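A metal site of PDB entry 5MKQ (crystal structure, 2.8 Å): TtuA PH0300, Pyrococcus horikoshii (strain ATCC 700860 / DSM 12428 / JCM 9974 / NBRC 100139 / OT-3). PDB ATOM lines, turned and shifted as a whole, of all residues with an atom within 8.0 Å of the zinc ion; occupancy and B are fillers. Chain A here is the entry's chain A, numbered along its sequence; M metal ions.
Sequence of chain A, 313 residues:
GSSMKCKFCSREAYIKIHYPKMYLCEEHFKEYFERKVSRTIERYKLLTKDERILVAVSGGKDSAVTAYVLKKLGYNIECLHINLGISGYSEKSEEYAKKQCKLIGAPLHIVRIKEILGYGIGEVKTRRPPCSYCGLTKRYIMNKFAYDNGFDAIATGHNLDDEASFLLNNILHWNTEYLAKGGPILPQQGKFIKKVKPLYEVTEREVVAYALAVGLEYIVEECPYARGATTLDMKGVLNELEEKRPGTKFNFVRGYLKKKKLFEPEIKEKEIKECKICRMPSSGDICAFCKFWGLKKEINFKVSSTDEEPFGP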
ATOM      1  N   TYR A 140      10.516 -26.624  15.355  1.00  0.00           N
ATOM      2  CA  TYR A 140      10.958 -27.536  16.394  1.00  0.00           C
ATOM      3  C   TYR A 140      10.361 -28.920  16.193  1.00  0.00           C
ATOM      4  O   TYR A 140      11.112 -29.898  16.198  1.00  0.00           O
ATOM      5  CB  TYR A 140      10.631 -27.010  17.803  1.00  0.00           C
ATOM      6  CG  TYR A 140      10.961 -28.000  18.903  1.00  0.00           C
ATOM      7  CD1 TYR A 140      10.049 -28.976  19.291  1.00  0.00           C
ATOM      8  CD2 TYR A 140      12.203 -27.986  19.542  1.00  0.00           C
ATOM      9  CE1 TYR A 140      10.352 -29.909  20.288  1.00  0.00           C
ATOM     10  CE2 TYR A 140      12.516 -28.901  20.548  1.00  0.00           C
ATOM     11  CZ  TYR A 140      11.581 -29.860  20.925  1.00  0.00           C
ATOM     12  OH  TYR A 140      11.877 -30.760  21.906  1.00  0.00           O
ATOM     13  N   LYS A 144      12.343 -32.312  15.486  1.00  0.00           N
ATOM     14  CA  LYS A 144      12.262 -33.326  16.548  1.00  0.00           C
ATOM     15  C   LYS A 144      11.582 -34.602  16.054  1.00  0.00           C
ATOM     16  O   LYS A 144      12.031 -35.697  16.390  1.00  0.00           O
ATOM     17  CB  LYS A 144      11.589 -32.754  17.810  1.00  0.00           C
ATOM     18  CG  LYS A 144      11.615 -33.647  19.055  1.00  0.00           C
ATOM     19  CD  LYS A 144      12.910 -33.612  19.848  1.00  0.00           C
ATOM     20  CE  LYS A 144      12.733 -34.029  21.296  1.00  0.00           C
ATOM     21  NZ  LYS A 144      12.412 -35.473  21.452  1.00  0.00           N
ATOM     22  N   GLU A 274      23.442 -27.610  24.237  1.00  0.00           N
ATOM     23  CA  GLU A 274      22.410 -28.659  24.201  1.00  0.00           C
ATOM     24  C   GLU A 274      21.405 -28.368  25.326  1.00  0.00           C
ATOM     25  O   GLU A 274      21.820 -28.097  26.459  1.00  0.00           O
ATOM     26  CB  GLU A 274      23.012 -30.068  24.360  1.00  0.00           C
ATOM     27  CG  GLU A 274      24.065 -30.443  23.327  1.00  0.00           C
ATOM     28  CD  GLU A 274      25.457 -29.862  23.564  1.00  0.00           C
ATOM     29  OE1 GLU A 274      26.060 -30.141  24.614  1.00  0.00           O
ATOM     30  OE2 GLU A 274      25.937 -29.119  22.671  1.00  0.00           O
ATOM     31  N   CYS A 275      20.100 -28.425  25.013  1.00  0.00           N
ATOM     32  CA  CYS A 275      19.023 -28.150  25.960  1.00  0.00           C
ATOM     33  C   CYS A 275      19.065 -29.037  27.210  1.00  0.00           C
ATOM     34  O   CYS A 275      19.408 -30.209  27.127  1.00  0.00           O
ATOM     35  CB  CYS A 275      17.654 -28.190  25.284  1.00  0.00           C
ATOM     36  SG  CYS A 275      16.267 -27.805  26.380  1.00  0.00           S
ATOM     37  N   LYS A 276      18.712 -28.451  28.363  1.00  0.00           N
ATOM     38  CA  LYS A 276      18.669 -29.112  29.668  1.00  0.00           C
ATOM     39  C   LYS A 276      17.423 -30.027  29.798  1.00  0.00           C
ATOM     40  O   LYS A 276      17.396 -30.908  30.654  1.00  0.00           O
ATOM     41  CB  LYS A 276      18.678 -28.030  30.770  1.00  0.00           C
ATOM     42  CG  LYS A 276      19.191 -28.491  32.135  1.00  0.00           C
ATOM     43  CD  LYS A 276      19.136 -27.361  33.158  1.00  0.00           C
ATOM     44  CE  LYS A 276      19.698 -27.775  34.497  1.00  0.00           C
ATOM     45  NZ  LYS A 276      19.656 -26.671  35.491  1.00  0.00           N
ATOM     46  N   ILE A 277      16.389 -29.799  28.942  1.00  0.00           N
ATOM     47  CA  ILE A 277      15.110 -30.520  28.961  1.00  0.00           C
ATOM     48  C   ILE A 277      14.978 -31.566  27.838  1.00  0.00           C
ATOM     49  O   ILE A 277      14.777 -32.749  28.131  1.00  0.00           O
ATOM     50  CB  ILE A 277      13.896 -29.527  28.976  1.00  0.00           C
ATOM     51  CG1 ILE A 277      14.034 -28.411  30.060  1.00  0.00           C
ATOM     52  CG2 ILE A 277      12.549 -30.266  29.087  1.00  0.00           C
ATOM     53  CD1 ILE A 277      14.093 -28.834  31.583  1.00  0.00           C
ATOM     54  N   CYS A 278      15.024 -31.123  26.567  1.00  0.00           N
ATOM     55  CA  CYS A 278      14.840 -31.988  25.404  1.00  0.00           C
ATOM     56  C   CYS A 278      16.147 -32.457  24.758  1.00  0.00           C
ATOM     57  O   CYS A 278      16.099 -33.321  23.876  1.00  0.00           O
ATOM     58  CB  CYS A 278      13.926 -31.321  24.375  1.00  0.00           C
ATOM     59  SG  CYS A 278      14.590 -29.768  23.707  1.00  0.00           S
ATOM     60  N   ARG A 279      17.297 -31.880  25.170  1.00  0.00           N
ATOM     61  CA  ARG A 279      18.658 -32.151  24.682  1.00  0.00           C
ATOM     62  C   ARG A 279      18.853 -31.709  23.207  1.00  0.00           C
ATOM     63  O   ARG A 279      19.870 -32.048  22.583  1.00  0.00           O
ATOM     64  CB  ARG A 279      19.114 -33.607  24.907  1.00  0.00           C
ATOM     65  CG  ARG A 279      18.973 -34.130  26.330  1.00  0.00           C
ATOM     66  CD  ARG A 279      18.659 -35.622  26.382  1.00  0.00           C
ATOM     67  NE  ARG A 279      19.767 -36.407  26.929  1.00  0.00           N
ATOM     68  CZ  ARG A 279      19.968 -36.641  28.226  1.00  0.00           C
ATOM     69  NH1 ARG A 279      19.145 -36.120  29.133  1.00  0.00           N
ATOM     70  NH2 ARG A 279      20.994 -37.374  28.627  1.00  0.00           N
ATOM     71  N   MET A 280      17.910 -30.900  22.680  1.00  0.00           N
ATOM     72  CA  MET A 280      17.971 -30.382  21.312  1.00  0.00           C
ATOM     73  C   MET A 280      18.904 -29.162  21.208  1.00  0.00           C
ATOM     74  O   MET A 280      19.149 -28.530  22.238  1.00  0.00           O
ATOM     75  CB  MET A 280      16.558 -30.070  20.772  1.00  0.00           C
ATOM     76  CG  MET A 280      15.703 -31.304  20.549  1.00  0.00           C
ATOM     77  SD  MET A 280      16.442 -32.638  19.572  1.00  0.00           S
ATOM     78  CE  MET A 280      16.397 -31.931  17.927  1.00  0.00           C
ATOM     79  N   PRO A 281      19.466 -28.842  20.006  1.00  0.00           N
ATOM     80  CA  PRO A 281      20.397 -27.705  19.906  1.00  0.00           C
ATOM     81  C   PRO A 281      19.852 -26.371  20.445  1.00  0.00           C
ATOM     82  O   PRO A 281      18.923 -25.788  19.882  1.00  0.00           O
ATOM     83  CB  PRO A 281      20.755 -27.647  18.407  1.00  0.00           C
ATOM     84  CG  PRO A 281      19.752 -28.498  17.725  1.00  0.00           C
ATOM     85  CD  PRO A 281      19.323 -29.525  18.702  1.00  0.00           C
ATOM     86  N   SER A 282      20.443 -25.934  21.575  1.00  0.00           N
ATOM     87  CA  SER A 282      20.102 -24.728  22.333  1.00  0.00           C
ATOM     88  C   SER A 282      21.219 -23.666  22.270  1.00  0.00           C
ATOM     89  O   SER A 282      22.368 -23.992  21.962  1.00  0.00           O
ATOM     90  CB  SER A 282      19.803 -25.098  23.780  1.00  0.00           C
ATOM     91  OG  SER A 282      19.584 -23.967  24.612  1.00  0.00           O
ATOM     92  N   ASP A 285      21.090 -22.393  28.417  1.00  0.00           N
ATOM     93  CA  ASP A 285      20.859 -23.590  29.242  1.00  0.00           C
ATOM     94  C   ASP A 285      19.664 -24.418  28.729  1.00  0.00           C
ATOM     95  O   ASP A 285      19.767 -25.635  28.600  1.00  0.00           O
ATOM     96  CB  ASP A 285      20.678 -23.200  30.719  1.00  0.00           C
ATOM     97  CG  ASP A 285      21.791 -23.681  31.628  1.00  0.00           C
ATOM     98  OD1 ASP A 285      22.872 -23.056  31.617  1.00  0.00           O
ATOM     99  OD2 ASP A 285      21.568 -24.663  32.371  1.00  0.00           O
ATOM    100  N   ILE A 286      18.533 -23.743  28.441  1.00  0.00           N
ATOM    101  CA  ILE A 286      17.283 -24.314  27.952  1.00  0.00           C
ATOM    102  C   ILE A 286      16.971 -23.684  26.584  1.00  0.00           C
ATOM    103  O   ILE A 286      17.205 -22.486  26.409  1.00  0.00           O
ATOM    104  CB  ILE A 286      16.150 -24.122  29.012  1.00  0.00           C
ATOM    105  CG1 ILE A 286      16.432 -24.967  30.286  1.00  0.00           C
ATOM    106  CG2 ILE A 286      14.754 -24.443  28.453  1.00  0.00           C
ATOM    107  CD1 ILE A 286      15.978 -24.354  31.603  1.00  0.00           C
ATOM    108  N   CYS A 287      16.502 -24.487  25.610  1.00  0.00           N
ATOM    109  CA  CYS A 287      16.190 -24.013  24.251  1.00  0.00           C
ATOM    110  C   CYS A 287      14.988 -23.067  24.201  1.00  0.00           C
ATOM    111  O   CYS A 287      14.179 -23.041  25.135  1.00  0.00           O
ATOM    112  CB  CYS A 287      16.034 -25.182  23.267  1.00  0.00           C
ATOM    113  SG  CYS A 287      14.401 -25.964  23.275  1.00  0.00           S
ATOM    114  N   ALA A 288      14.891 -22.283  23.106  1.00  0.00           N
ATOM    115  CA  ALA A 288      13.816 -21.310  22.833  1.00  0.00           C
ATOM    116  C   ALA A 288      12.421 -21.931  22.930  1.00  0.00           C
ATOM    117  O   ALA A 288      11.518 -21.314  23.510  1.00  0.00           O
ATOM    118  CB  ALA A 288      14.027 -20.681  21.466  1.00  0.00           C
ATOM    119  N   PHE A 289      12.242 -23.140  22.387  1.00  0.00           N
ATOM    120  CA  PHE A 289      10.972 -23.875  22.412  1.00  0.00           C
ATOM    121  C   PHE A 289      10.607 -24.267  23.852  1.00  0.00           C
ATOM    122  O   PHE A 289       9.503 -23.960  24.303  1.00  0.00           O
ATOM    123  CB  PHE A 289      11.032 -25.107  21.497  1.00  0.00           C
ATOM    124  CG  PHE A 289       9.738 -25.881  21.365  1.00  0.00           C
ATOM    125  CD1 PHE A 289       8.811 -25.543  20.389  1.00  0.00           C
ATOM    126  CD2 PHE A 289       9.466 -26.961  22.196  1.00  0.00           C
ATOM    127  CE1 PHE A 289       7.627 -26.268  20.238  1.00  0.00           C
ATOM    128  CE2 PHE A 289       8.262 -27.669  22.066  1.00  0.00           C
ATOM    129  CZ  PHE A 289       7.360 -27.327  21.091  1.00  0.00           C
ATOM    130  N   CYS A 290      11.529 -24.926  24.586  1.00  0.00           N
ATOM    131  CA  CYS A 290      11.308 -25.354  25.964  1.00  0.00           C
ATOM    132  C   CYS A 290      11.105 -24.181  26.933  1.00  0.00           C
ATOM    133  O   CYS A 290      10.257 -24.281  27.817  1.00  0.00           O
ATOM    134  CB  CYS A 290      12.411 -26.296  26.434  1.00  0.00           C
ATOM    135  SG  CYS A 290      12.088 -28.060  26.118  1.00  0.00           S
ATOM    136  N   LYS A 291      11.863 -23.069  26.740  1.00  0.00           N
ATOM    137  CA  LYS A 291      11.734 -21.871  27.573  1.00  0.00           C
ATOM    138  C   LYS A 291      10.350 -21.229  27.430  1.00  0.00           C
ATOM    139  O   LYS A 291       9.722 -20.889  28.447  1.00  0.00           O
ATOM    140  CB  LYS A 291      12.895 -20.871  27.344  1.00  0.00           C
ATOM    141  CG  LYS A 291      12.763 -19.826  26.243  1.00  0.00           C
ATOM    142  CD  LYS A 291      13.990 -18.902  26.166  1.00  0.00           C
ATOM    143  CE  LYS A 291      13.795 -17.814  25.148  1.00  0.00           C
ATOM    144  NZ  LYS A 291      15.008 -16.974  24.972  1.00  0.00           N
ATOM    145  N   LEU A 295       8.353 -26.073  29.432  1.00  0.00           N
ATOM    146  CA  LEU A 295       8.398 -27.538  29.479  1.00  0.00           C
ATOM    147  C   LEU A 295       9.464 -28.076  30.424  1.00  0.00           C
ATOM    148  O   LEU A 295      10.625 -27.665  30.361  1.00  0.00           O
ATOM    149  CB  LEU A 295       8.566 -28.130  28.066  1.00  0.00           C
ATOM    150  CG  LEU A 295       7.547 -27.694  27.016  1.00  0.00           C
ATOM    151  CD1 LEU A 295       8.171 -27.638  25.656  1.00  0.00           C
ATOM    152  CD2 LEU A 295       6.324 -28.589  27.030  1.00  0.00           C
ATOM    153  N   LYS A 297       9.485 -31.662  30.858  1.00  0.00           N
ATOM    154  CA  LYS A 297       9.699 -32.982  30.229  1.00  0.00           C
ATOM    155  C   LYS A 297       9.950 -32.861  28.725  1.00  0.00           C
ATOM    156  O   LYS A 297       9.585 -31.842  28.119  1.00  0.00           O
ATOM    157  CB  LYS A 297       8.510 -33.910  30.497  1.00  0.00           C
ATOM    158  CG  LYS A 297       8.607 -34.697  31.798  1.00  0.00           C
ATOM    159  CD  LYS A 297       7.586 -35.821  31.816  1.00  0.00           C
ATOM    160  CE  LYS A 297       7.552 -36.525  33.147  1.00  0.00           C
ATOM    161  NZ  LYS A 297       6.517 -37.602  33.175  1.00  0.00           N
ATOM    162  N   GLU A 298      10.555 -33.900  28.134  1.00  0.00           N
ATOM    163  CA  GLU A 298      10.865 -33.972  26.696  1.00  0.00           C
ATOM    164  C   GLU A 298       9.717 -34.636  25.939  1.00  0.00           C
ATOM    165  O   GLU A 298       9.273 -35.721  26.331  1.00  0.00           O
ATOM    166  CB  GLU A 298      12.194 -34.725  26.483  1.00  0.00           C
ATOM    167  CG  GLU A 298      12.591 -34.919  25.020  1.00  0.00           C
ATOM    168  CD  GLU A 298      13.904 -35.637  24.773  1.00  0.00           C
ATOM    169  OE1 GLU A 298      14.748 -35.733  25.697  1.00  0.00           O
ATOM    170  OE2 GLU A 298      14.104 -36.094  23.619  1.00  0.00           O
HETATM  171 ZN    ZN M   1      14.367 -27.765  24.649  1.00  0.00          ZN
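The side-chain hydroxyl (OH) of Tyr 140 lies close to the side-chain sulfur (SG) of Cys 278 (3.4 Å). The side-chain sulfur (SG) of Cys 278 sits close to the backbone NH (N) of Met 280. The backbone NH of Phe 289 sits close to the side-chain sulfur of Cys 287, 3.7 Å away. The backbone NH of Cys 287 sits at hydrogen-bond distance from the side-chain hydroxyl of Ser 282. The backbone NH (N) of Ile 277 lies close to the side-chain sulfur (SG) of Cys 275, at 3.2 Å. The backbone carbonyl oxygen (O) of Met 280 sits at hydrogen-bond distance from the backbone NH (N) of Cys 275, at 2.9 Å. The backbone carbonyl oxygen (O) of Cys 290 lies within hydrogen-bond range of the backbone NH (N) of Leu 295 (3.1 Å).
Four residues have an atom within 4 Å of the zinc ion: Cys 275, Cys 278, Cys 287 and Cys 290. Along chain A the residues within 4 Å of the zinc ion span positions 275 to 290.
SG of Cys 278 binds the zinc ion, 2.2 Å away. The zinc ion is bound by SG of Cys 287. The zinc ion is bound by SG of Cys 275. The zinc ion is bound by the side-chain sulfur (SG) of Cys 290 (2.7 Å).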
